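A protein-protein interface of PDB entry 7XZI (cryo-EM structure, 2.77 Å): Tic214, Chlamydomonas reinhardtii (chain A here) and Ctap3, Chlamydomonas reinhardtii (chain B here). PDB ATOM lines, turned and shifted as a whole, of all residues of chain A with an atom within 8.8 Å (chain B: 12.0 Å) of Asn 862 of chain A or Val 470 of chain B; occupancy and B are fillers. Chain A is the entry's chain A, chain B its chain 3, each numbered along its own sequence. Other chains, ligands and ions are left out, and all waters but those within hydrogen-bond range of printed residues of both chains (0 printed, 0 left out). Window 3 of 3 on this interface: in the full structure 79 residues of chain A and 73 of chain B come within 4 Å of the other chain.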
ATOM      1  N   LEU A 859      -1.864  14.457  -3.030  1.00  0.00           N
ATOM      2  CA  LEU A 859      -1.704  13.259  -3.840  1.00  0.00           C
ATOM      3  C   LEU A 859      -0.274  13.141  -4.341  1.00  0.00           C
ATOM      4  O   LEU A 859       0.409  14.142  -4.569  1.00  0.00           O
ATOM      5  CB  LEU A 859      -2.661  13.258  -5.039  1.00  0.00           C
ATOM      6  CG  LEU A 859      -4.158  13.169  -4.749  1.00  0.00           C
ATOM      7  CD1 LEU A 859      -4.952  13.338  -6.031  1.00  0.00           C
ATOM      8  CD2 LEU A 859      -4.490  11.846  -4.085  1.00  0.00           C
ATOM      9  N   THR A 860       0.172  11.898  -4.503  1.00  0.00           N
ATOM     10  CA  THR A 860       1.440  11.617  -5.153  1.00  0.00           C
ATOM     11  C   THR A 860       1.271  11.672  -6.672  1.00  0.00           C
ATOM     12  O   THR A 860       0.160  11.615  -7.205  1.00  0.00           O
ATOM     13  CB  THR A 860       1.975  10.252  -4.716  1.00  0.00           C
ATOM     14  OG1 THR A 860       1.585   9.996  -3.364  1.00  0.00           O
ATOM     15  CG2 THR A 860       3.494  10.223  -4.795  1.00  0.00           C
ATOM     16  N   LYS A 861       2.401  11.792  -7.374  1.00  0.00           N
ATOM     17  CA  LYS A 861       2.365  11.855  -8.832  1.00  0.00           C
ATOM     18  C   LYS A 861       1.827  10.560  -9.432  1.00  0.00           C
ATOM     19  O   LYS A 861       1.032  10.590 -10.380  1.00  0.00           O
ATOM     20  CB  LYS A 861       3.760  12.165  -9.372  1.00  0.00           C
ATOM     21  CG  LYS A 861       4.258  13.549  -8.999  1.00  0.00           C
ATOM     22  CD  LYS A 861       5.691  13.781  -9.446  1.00  0.00           C
ATOM     23  CE  LYS A 861       6.681  13.041  -8.561  1.00  0.00           C
ATOM     24  NZ  LYS A 861       8.087  13.364  -8.929  1.00  0.00           N
ATOM     25  N   ASN A 862       2.251   9.415  -8.892  1.00  0.00           N
ATOM     26  CA  ASN A 862       1.743   8.138  -9.380  1.00  0.00           C
ATOM     27  C   ASN A 862       0.242   8.023  -9.162  1.00  0.00           C
ATOM     28  O   ASN A 862      -0.478   7.516 -10.028  1.00  0.00           O
ATOM     29  CB  ASN A 862       2.476   6.984  -8.700  1.00  0.00           C
ATOM     30  CG  ASN A 862       3.935   6.910  -9.094  1.00  0.00           C
ATOM     31  OD1 ASN A 862       4.326   7.385 -10.159  1.00  0.00           O
ATOM     32  ND2 ASN A 862       4.749   6.309  -8.236  1.00  0.00           N
ATOM     33  N   GLU A 863      -0.251   8.492  -8.012  1.00  0.00           N
ATOM     34  CA  GLU A 863      -1.687   8.452  -7.757  1.00  0.00           C
ATOM     35  C   GLU A 863      -2.446   9.350  -8.727  1.00  0.00           C
ATOM     36  O   GLU A 863      -3.527   8.987  -9.200  1.00  0.00           O
ATOM     37  CB  GLU A 863      -1.977   8.847  -6.309  1.00  0.00           C
ATOM     38  CG  GLU A 863      -1.406   7.881  -5.276  1.00  0.00           C
ATOM     39  CD  GLU A 863      -1.833   8.211  -3.857  1.00  0.00           C
ATOM     40  OE1 GLU A 863      -2.412   9.297  -3.645  1.00  0.00           O
ATOM     41  OE2 GLU A 863      -1.593   7.384  -2.953  1.00  0.00           O
ATOM     42  N   GLU A 864      -1.896  10.527  -9.035  1.00  0.00           N
ATOM     43  CA  GLU A 864      -2.543  11.417  -9.997  1.00  0.00           C
ATOM     44  C   GLU A 864      -2.595  10.790 -11.387  1.00  0.00           C
ATOM     45  O   GLU A 864      -3.626  10.860 -12.070  1.00  0.00           O
ATOM     46  CB  GLU A 864      -1.813  12.759 -10.038  1.00  0.00           C
ATOM     47  CG  GLU A 864      -2.441  13.784 -10.966  1.00  0.00           C
ATOM     48  CD  GLU A 864      -3.823  14.206 -10.514  1.00  0.00           C
ATOM     49  OE1 GLU A 864      -3.994  14.498  -9.312  1.00  0.00           O
ATOM     50  OE2 GLU A 864      -4.740  14.242 -11.361  1.00  0.00           O
ATOM     51  N   ARG A 865      -1.494  10.171 -11.822  1.00  0.00           N
ATOM     52  CA  ARG A 865      -1.503   9.487 -13.110  1.00  0.00           C
ATOM     53  C   ARG A 865      -2.483   8.324 -13.124  1.00  0.00           C
ATOM     54  O   ARG A 865      -3.175   8.111 -14.127  1.00  0.00           O
ATOM     55  CB  ARG A 865      -0.098   8.997 -13.465  1.00  0.00           C
ATOM     56  CG  ARG A 865       0.854  10.103 -13.888  1.00  0.00           C
ATOM     57  CD  ARG A 865       2.136   9.538 -14.473  1.00  0.00           C
ATOM     58  NE  ARG A 865       3.004   8.973 -13.450  1.00  0.00           N
ATOM     59  CZ  ARG A 865       3.993   9.634 -12.858  1.00  0.00           C
ATOM     60  NH1 ARG A 865       4.270  10.888 -13.172  1.00  0.00           N
ATOM     61  NH2 ARG A 865       4.718   9.020 -11.929  1.00  0.00           N
ATOM     62  N   ALA A 866      -2.559   7.572 -12.024  1.00  0.00           N
ATOM     63  CA  ALA A 866      -3.523   6.482 -11.929  1.00  0.00           C
ATOM     64  C   ALA A 866      -4.951   7.000 -12.010  1.00  0.00           C
ATOM     65  O   ALA A 866      -5.805   6.376 -12.646  1.00  0.00           O
ATOM     66  CB  ALA A 866      -3.306   5.702 -10.633  1.00  0.00           C
ATOM     67  N   LEU A 867      -5.233   8.133 -11.362  1.00  0.00           N
ATOM     68  CA  LEU A 867      -6.567   8.720 -11.445  1.00  0.00           C
ATOM     69  C   LEU A 867      -6.889   9.162 -12.867  1.00  0.00           C
ATOM     70  O   LEU A 867      -8.015   8.971 -13.340  1.00  0.00           O
ATOM     71  CB  LEU A 867      -6.690   9.896 -10.475  1.00  0.00           C
ATOM     72  CG  LEU A 867      -6.665   9.587  -8.976  1.00  0.00           C
ATOM     73  CD1 LEU A 867      -6.837  10.856  -8.155  1.00  0.00           C
ATOM     74  CD2 LEU A 867      -7.733   8.567  -8.618  1.00  0.00           C
ATOM     75  N   HIS A 868      -5.919   9.759 -13.563  1.00  0.00           N
ATOM     76  CA  HIS A 868      -6.132  10.146 -14.958  1.00  0.00           C
ATOM     77  C   HIS A 868      -6.443   8.927 -15.825  1.00  0.00           C
ATOM     78  O   HIS A 868      -7.380   8.937 -16.642  1.00  0.00           O
ATOM     79  CB  HIS A 868      -4.896  10.885 -15.478  1.00  0.00           C
ATOM     80  CG  HIS A 868      -5.021  11.366 -16.890  1.00  0.00           C
ATOM     81  ND1 HIS A 868      -6.082  12.130 -17.326  1.00  0.00           N
ATOM     82  CD2 HIS A 868      -4.210  11.203 -17.962  1.00  0.00           C
ATOM     83  CE1 HIS A 868      -5.925  12.411 -18.607  1.00  0.00           C
ATOM     84  NE2 HIS A 868      -4.796  11.860 -19.017  1.00  0.00           N
ATOM     85  N   ILE A 869      -5.661   7.858 -15.647  1.00  0.00           N
ATOM     86  CA  ILE A 869      -5.877   6.633 -16.410  1.00  0.00           C
ATOM     87  C   ILE A 869      -7.243   6.040 -16.092  1.00  0.00           C
ATOM     88  O   ILE A 869      -7.960   5.579 -16.989  1.00  0.00           O
ATOM     89  CB  ILE A 869      -4.739   5.628 -16.145  1.00  0.00           C
ATOM     90  CG1 ILE A 869      -3.397   6.200 -16.611  1.00  0.00           C
ATOM     91  CG2 ILE A 869      -5.011   4.317 -16.853  1.00  0.00           C
ATOM     92  CD1 ILE A 869      -2.218   5.286 -16.346  1.00  0.00           C
ATOM     93  N   ARG A 870      -7.627   6.040 -14.813  1.00  0.00           N
ATOM     94  CA  ARG A 870      -8.941   5.537 -14.429  1.00  0.00           C
ATOM     95  C   ARG A 870     -10.051   6.350 -15.075  1.00  0.00           C
ATOM     96  O   ARG A 870     -11.041   5.787 -15.551  1.00  0.00           O
ATOM     97  CB  ARG A 870      -9.101   5.559 -12.910  1.00  0.00           C
ATOM     98  CG  ARG A 870      -8.379   4.456 -12.164  1.00  0.00           C
ATOM     99  CD  ARG A 870      -8.882   4.395 -10.731  1.00  0.00           C
ATOM    100  NE  ARG A 870      -8.246   3.340  -9.954  1.00  0.00           N
ATOM    101  CZ  ARG A 870      -7.238   3.535  -9.113  1.00  0.00           C
ATOM    102  NH1 ARG A 870      -6.715   4.735  -8.926  1.00  0.00           N
ATOM    103  NH2 ARG A 870      -6.747   2.500  -8.440  1.00  0.00           N
ATOM    104  N   GLY A 930       7.517  14.343 -18.456  1.00  0.00           N
ATOM    105  CA  GLY A 930       8.407  13.835 -17.434  1.00  0.00           C
ATOM    106  C   GLY A 930       7.648  13.553 -16.154  1.00  0.00           C
ATOM    107  O   GLY A 930       6.416  13.574 -16.118  1.00  0.00           O
ATOM    108  N   ASP A 931       8.419  13.288 -15.099  1.00  0.00           N
ATOM    109  CA  ASP A 931       7.865  12.977 -13.782  1.00  0.00           C
ATOM    110  C   ASP A 931       7.647  14.278 -13.006  1.00  0.00           C
ATOM    111  O   ASP A 931       8.362  14.615 -12.061  1.00  0.00           O
ATOM    112  CB  ASP A 931       8.784  12.021 -13.035  1.00  0.00           C
ATOM    113  CG  ASP A 931       8.136  11.434 -11.800  1.00  0.00           C
ATOM    114  OD1 ASP A 931       6.918  11.637 -11.609  1.00  0.00           O
ATOM    115  OD2 ASP A 931       8.843  10.766 -11.017  1.00  0.00           O
ATOM    116  N   PHE A 932       6.626  15.019 -13.430  1.00  0.00           N
ATOM    117  CA  PHE A 932       6.284  16.296 -12.825  1.00  0.00           C
ATOM    118  C   PHE A 932       4.783  16.365 -12.586  1.00  0.00           C
ATOM    119  O   PHE A 932       4.003  15.610 -13.171  1.00  0.00           O
ATOM    120  CB  PHE A 932       6.716  17.481 -13.703  1.00  0.00           C
ATOM    121  CG  PHE A 932       8.156  17.443 -14.116  1.00  0.00           C
ATOM    122  CD1 PHE A 932       9.162  17.686 -13.198  1.00  0.00           C
ATOM    123  CD2 PHE A 932       8.505  17.178 -15.430  1.00  0.00           C
ATOM    124  CE1 PHE A 932      10.488  17.656 -13.578  1.00  0.00           C
ATOM    125  CE2 PHE A 932       9.830  17.146 -15.816  1.00  0.00           C
ATOM    126  CZ  PHE A 932      10.823  17.385 -14.889  1.00  0.00           C
ATOM    127  N   TYR A 933       4.387  17.284 -11.710  1.00  0.00           N
ATOM    128  CA  TYR A 933       2.977  17.598 -11.522  1.00  0.00           C
ATOM    129  C   TYR A 933       2.498  18.438 -12.698  1.00  0.00           C
ATOM    130  O   TYR A 933       3.043  19.516 -12.958  1.00  0.00           O
ATOM    131  CB  TYR A 933       2.757  18.345 -10.210  1.00  0.00           C
ATOM    132  CG  TYR A 933       2.887  17.485  -8.977  1.00  0.00           C
ATOM    133  CD1 TYR A 933       1.801  16.775  -8.490  1.00  0.00           C
ATOM    134  CD2 TYR A 933       4.091  17.391  -8.296  1.00  0.00           C
ATOM    135  CE1 TYR A 933       1.910  15.991  -7.362  1.00  0.00           C
ATOM    136  CE2 TYR A 933       4.211  16.608  -7.167  1.00  0.00           C
ATOM    137  CZ  TYR A 933       3.117  15.911  -6.704  1.00  0.00           C
ATOM    138  OH  TYR A 933       3.228  15.128  -5.579  1.00  0.00           O
ATOM    139  N   TYR A 942      -9.513  10.702  -4.223  1.00  0.00           N
ATOM    140  CA  TYR A 942     -10.009   9.452  -3.666  1.00  0.00           C
ATOM    141  C   TYR A 942     -11.074   9.738  -2.616  1.00  0.00           C
ATOM    142  O   TYR A 942     -11.039  10.765  -1.933  1.00  0.00           O
ATOM    143  CB  TYR A 942      -8.878   8.641  -3.029  1.00  0.00           C
ATOM    144  CG  TYR A 942      -7.931   7.982  -4.003  1.00  0.00           C
ATOM    145  CD1 TYR A 942      -8.298   6.834  -4.691  1.00  0.00           C
ATOM    146  CD2 TYR A 942      -6.658   8.492  -4.218  1.00  0.00           C
ATOM    147  CE1 TYR A 942      -7.432   6.223  -5.576  1.00  0.00           C
ATOM    148  CE2 TYR A 942      -5.785   7.888  -5.101  1.00  0.00           C
ATOM    149  CZ  TYR A 942      -6.177   6.753  -5.777  1.00  0.00           C
ATOM    150  OH  TYR A 942      -5.313   6.146  -6.657  1.00  0.00           O
ATOM    151  N   GLY B 409      13.571   9.388 -22.817  1.00  0.00           N
ATOM    152  CA  GLY B 409      14.251   8.829 -21.667  1.00  0.00           C
ATOM    153  C   GLY B 409      13.635   7.517 -21.235  1.00  0.00           C
ATOM    154  O   GLY B 409      12.775   6.979 -21.936  1.00  0.00           O
ATOM    155  N   GLN B 410      14.059   6.991 -20.084  1.00  0.00           N
ATOM    156  CA  GLN B 410      13.515   5.723 -19.608  1.00  0.00           C
ATOM    157  C   GLN B 410      12.038   5.841 -19.251  1.00  0.00           C
ATOM    158  O   GLN B 410      11.276   4.887 -19.447  1.00  0.00           O
ATOM    159  CB  GLN B 410      14.317   5.226 -18.407  1.00  0.00           C
ATOM    160  CG  GLN B 410      13.844   3.894 -17.849  1.00  0.00           C
ATOM    161  CD  GLN B 410      14.682   3.423 -16.679  1.00  0.00           C
ATOM    162  OE1 GLN B 410      15.734   3.990 -16.388  1.00  0.00           O
ATOM    163  NE2 GLN B 410      14.218   2.381 -16.001  1.00  0.00           N
ATOM    164  N   TYR B 411      11.618   6.993 -18.736  1.00  0.00           N
ATOM    165  CA  TYR B 411      10.222   7.199 -18.369  1.00  0.00           C
ATOM    166  C   TYR B 411       9.354   7.237 -19.622  1.00  0.00           C
ATOM    167  O   TYR B 411       9.521   8.117 -20.474  1.00  0.00           O
ATOM    168  CB  TYR B 411      10.083   8.493 -17.571  1.00  0.00           C
ATOM    169  CG  TYR B 411       8.659   8.884 -17.252  1.00  0.00           C
ATOM    170  CD1 TYR B 411       7.971   8.283 -16.206  1.00  0.00           C
ATOM    171  CD2 TYR B 411       8.007   9.864 -17.987  1.00  0.00           C
ATOM    172  CE1 TYR B 411       6.671   8.641 -15.909  1.00  0.00           C
ATOM    173  CE2 TYR B 411       6.707  10.227 -17.697  1.00  0.00           C
ATOM    174  CZ  TYR B 411       6.045   9.613 -16.656  1.00  0.00           C
ATOM    175  OH  TYR B 411       4.750   9.973 -16.364  1.00  0.00           O
ATOM    176  N   MET B 412       8.425   6.288 -19.727  1.00  0.00           N
ATOM    177  CA  MET B 412       7.553   6.137 -20.892  1.00  0.00           C
ATOM    178  C   MET B 412       8.379   6.050 -22.176  1.00  0.00           C
ATOM    179  O   MET B 412       8.284   6.885 -23.078  1.00  0.00           O
ATOM    180  CB  MET B 412       6.528   7.274 -20.958  1.00  0.00           C
ATOM    181  CG  MET B 412       5.620   7.353 -19.740  1.00  0.00           C
ATOM    182  SD  MET B 412       4.387   8.664 -19.853  1.00  0.00           S
ATOM    183  CE  MET B 412       3.502   8.170 -21.327  1.00  0.00           C
ATOM    184  N   ALA B 413       9.202   5.003 -22.239  1.00  0.00           N
ATOM    185  CA  ALA B 413      10.185   4.836 -23.301  1.00  0.00           C
ATOM    186  C   ALA B 413       9.741   3.903 -24.416  1.00  0.00           C
ATOM    187  O   ALA B 413      10.248   4.020 -25.537  1.00  0.00           O
ATOM    188  CB  ALA B 413      11.498   4.298 -22.721  1.00  0.00           C
ATOM    189  N   GLY B 414       8.812   2.996 -24.147  1.00  0.00           N
ATOM    190  CA  GLY B 414       8.545   1.899 -25.051  1.00  0.00           C
ATOM    191  C   GLY B 414       9.308   0.645 -24.660  1.00  0.00           C
ATOM    192  O   GLY B 414      10.244   0.667 -23.863  1.00  0.00           O
ATOM    193  N   ALA B 418      13.421   1.266 -23.568  1.00  0.00           N
ATOM    194  CA  ALA B 418      13.718   1.156 -22.144  1.00  0.00           C
ATOM    195  C   ALA B 418      14.754   0.072 -21.880  1.00  0.00           C
ATOM    196  O   ALA B 418      15.690   0.275 -21.098  1.00  0.00           O
ATOM    197  CB  ALA B 418      12.436   0.876 -21.360  1.00  0.00           C
ATOM    198  N   ILE B 422      18.479   0.609 -20.360  1.00  0.00           N
ATOM    199  CA  ILE B 422      18.896  -0.113 -19.161  1.00  0.00           C
ATOM    200  C   ILE B 422      20.199  -0.860 -19.415  1.00  0.00           C
ATOM    201  O   ILE B 422      21.121  -0.830 -18.589  1.00  0.00           O
ATOM    202  CB  ILE B 422      17.778  -1.062 -18.691  1.00  0.00           C
ATOM    203  CG1 ILE B 422      16.604  -0.265 -18.119  1.00  0.00           C
ATOM    204  CG2 ILE B 422      18.307  -2.046 -17.659  1.00  0.00           C
ATOM    205  CD1 ILE B 422      15.451  -1.127 -17.655  1.00  0.00           C
ATOM    206  N   VAL B 463       0.776  -0.401 -23.679  1.00  0.00           N
ATOM    207  CA  VAL B 463       2.174  -0.241 -23.290  1.00  0.00           C
ATOM    208  C   VAL B 463       2.380   1.088 -22.577  1.00  0.00           C
ATOM    209  O   VAL B 463       3.097   1.167 -21.570  1.00  0.00           O
ATOM    210  CB  VAL B 463       3.087  -0.375 -24.523  1.00  0.00           C
ATOM    211  CG1 VAL B 463       4.540  -0.168 -24.132  1.00  0.00           C
ATOM    212  CG2 VAL B 463       2.894  -1.735 -25.172  1.00  0.00           C
ATOM    213  N   ALA B 464       1.760   2.155 -23.088  1.00  0.00           N
ATOM    214  CA  ALA B 464       1.897   3.465 -22.460  1.00  0.00           C
ATOM    215  C   ALA B 464       1.354   3.452 -21.036  1.00  0.00           C
ATOM    216  O   ALA B 464       1.966   4.010 -20.119  1.00  0.00           O
ATOM    217  CB  ALA B 464       1.188   4.525 -23.301  1.00  0.00           C
ATOM    218  N   VAL B 465       0.195   2.821 -20.834  1.00  0.00           N
ATOM    219  CA  VAL B 465      -0.365   2.699 -19.492  1.00  0.00           C
ATOM    220  C   VAL B 465       0.542   1.863 -18.600  1.00  0.00           C
ATOM    221  O   VAL B 465       0.762   2.203 -17.431  1.00  0.00           O
ATOM    222  CB  VAL B 465      -1.788   2.113 -19.568  1.00  0.00           C
ATOM    223  CG1 VAL B 465      -2.285   1.737 -18.184  1.00  0.00           C
ATOM    224  CG2 VAL B 465      -2.727   3.116 -20.216  1.00  0.00           C
ATOM    225  N   GLY B 466       1.085   0.764 -19.129  1.00  0.00           N
ATOM    226  CA  GLY B 466       1.968  -0.074 -18.336  1.00  0.00           C
ATOM    227  C   GLY B 466       3.244   0.624 -17.913  1.00  0.00           C
ATOM    228  O   GLY B 466       3.777   0.350 -16.835  1.00  0.00           O
ATOM    229  N   GLY B 467       3.756   1.522 -18.749  1.00  0.00           N
ATOM    230  CA  GLY B 467       4.987   2.224 -18.438  1.00  0.00           C
ATOM    231  C   GLY B 467       4.764   3.575 -17.789  1.00  0.00           C
ATOM    232  O   GLY B 467       5.648   4.437 -17.813  1.00  0.00           O
ATOM    233  N   ALA B 468       3.579   3.777 -17.220  1.00  0.00           N
ATOM    234  CA  ALA B 468       3.197   5.060 -16.648  1.00  0.00           C
ATOM    235  C   ALA B 468       3.445   5.158 -15.148  1.00  0.00           C
ATOM    236  O   ALA B 468       3.145   6.201 -14.558  1.00  0.00           O
ATOM    237  CB  ALA B 468       1.719   5.342 -16.939  1.00  0.00           C
ATOM    238  N   PHE B 469       3.977   4.117 -14.513  1.00  0.00           N
ATOM    239  CA  PHE B 469       4.190   4.106 -13.071  1.00  0.00           C
ATOM    240  C   PHE B 469       5.673   3.938 -12.777  1.00  0.00           C
ATOM    241  O   PHE B 469       6.309   3.010 -13.287  1.00  0.00           O
ATOM    242  CB  PHE B 469       3.379   2.995 -12.402  1.00  0.00           C
ATOM    243  CG  PHE B 469       1.897   3.137 -12.586  1.00  0.00           C
ATOM    244  CD1 PHE B 469       1.193   4.114 -11.905  1.00  0.00           C
ATOM    245  CD2 PHE B 469       1.207   2.291 -13.438  1.00  0.00           C
ATOM    246  CE1 PHE B 469      -0.170   4.249 -12.071  1.00  0.00           C
ATOM    247  CE2 PHE B 469      -0.157   2.421 -13.609  1.00  0.00           C
ATOM    248  CZ  PHE B 469      -0.846   3.401 -12.925  1.00  0.00           C
ATOM    249  N   VAL B 470       6.214   4.830 -11.961  1.00  0.00           N
ATOM    250  CA  VAL B 470       7.615   4.787 -11.547  1.00  0.00           C
ATOM    251  C   VAL B 470       7.689   4.149 -10.165  1.00  0.00           C
ATOM    252  O   VAL B 470       7.031   4.639  -9.238  1.00  0.00           O
ATOM    253  CB  VAL B 470       8.245   6.191 -11.534  1.00  0.00           C
ATOM    254  CG1 VAL B 470       9.659   6.126 -10.981  1.00  0.00           C
ATOM    255  CG2 VAL B 470       8.242   6.787 -12.932  1.00  0.00           C
ATOM    256  N   PRO B 471       8.449   3.067  -9.989  1.00  0.00           N
ATOM    257  CA  PRO B 471       8.561   2.449  -8.661  1.00  0.00           C
ATOM    258  C   PRO B 471       9.199   3.404  -7.661  1.00  0.00           C
ATOM    259  O   PRO B 471      10.085   4.189  -8.008  1.00  0.00           O
ATOM    260  CB  PRO B 471       9.447   1.223  -8.913  1.00  0.00           C
ATOM    261  CG  PRO B 471      10.222   1.570 -10.143  1.00  0.00           C
ATOM    262  CD  PRO B 471       9.289   2.387 -10.989  1.00  0.00           C
ATOM    263  N   SER B 472       8.741   3.333  -6.416  1.00  0.00           N
ATOM    264  CA  SER B 472       9.258   4.196  -5.360  1.00  0.00           C
ATOM    265  C   SER B 472      10.476   3.572  -4.686  1.00  0.00           C
ATOM    266  O   SER B 472      11.588   4.088  -4.794  1.00  0.00           O
ATOM    267  CB  SER B 472       8.172   4.484  -4.322  1.00  0.00           C
ATOM    268  OG  SER B 472       7.044   5.099  -4.918  1.00  0.00           O
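OH of Tyr 411 of chain B lies close to NH1 of Arg 865 of chain A, 3.4 Å away.
The backbone carbonyl oxygen (O) of Ala 468 of chain B sits at hydrogen-bond distance from the guanidinium group (NE) of Arg 865 of chain A (3.0 Å).
The side-chain amide nitrogen (ND2) of Asn 862 of chain A lies within hydrogen-bond range of the backbone carbonyl oxygen (O) of Val 470 of chain B.
The side-chain hydroxyl (OH) of Tyr 411 of chain B lies close to the side-chain sulfur (SD) of Met 412 of chain B (3.7 Å).
The side-chain amide oxygen (OD1) of Asn 862 of chain A is in hydrogen-bond range of the guanidinium group (NH2) of Arg 865 of chain A (2.4 Å).
The guanidinium group of Arg 865 of chain A lies within salt-bridge range of the side-chain carboxylate of Asp 931 of chain A (3.2 Å).
Among the printed residues, merely in contact across the chains: Gly 930 of chain A with Tyr 411 of chain B, Ala 866 of chain A with Phe 469 of chain B, Asn 862 of chain A with Phe 469 of chain B, Ile 869 of chain A with Ala 468 of chain B and Ile 869 of chain A with Val 465 of chain B.
No residue of chain B comes within 4 Å of Thr 860 of chain A.
No residue of chain B comes within 4 Å of Lys 861 of chain A.
Of chain B, only Phe 469 (3.9 Å) and Val 470 (3.0 Å) come within 4 Å of Asn 862 of chain A.
No residue of chain B comes within 4 Å of Glu 863 of chain A.
Arg 865 of chain A touches two residues of chain B.
Ala 866 of chain A touches just one residue of chain B: Phe 469.
Of the printed residues of chain B, Ile 869 of chain A touches Val 465 and Ala 468.
Of the printed residues of chain B, Gly 930 of chain A touches Tyr 411 (3.7 Å).
Printed residues of chain A within 4 Å of Val 465 of chain B: Ile 869.
Gly 466 of chain B touches none of the printed residues of chain A.
Printed residues of chain A within 4 Å of Phe 469 of chain B: Asn 862 (3.9 Å) and Ala 866 (3.7 Å).
Printed residues of chain A within 4 Å of Val 470 of chain B: Asn 862.
Pro 471 of chain B touches none of the printed residues of chain A.
The nearest printed residue of chain B that does not touch Ile 869 of chain A is Phe 469 of chain B (4.1 Å).
Printed residues of chain A that touch a printed residue of chain B: Asn 862, Arg 865, Ala 866, Ile 869 and Gly 930.
Of the 18 printed residues of chain B, 5 touch a printed residue of chain A.
Among the printed residues, 8 pairs touch across the chains.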
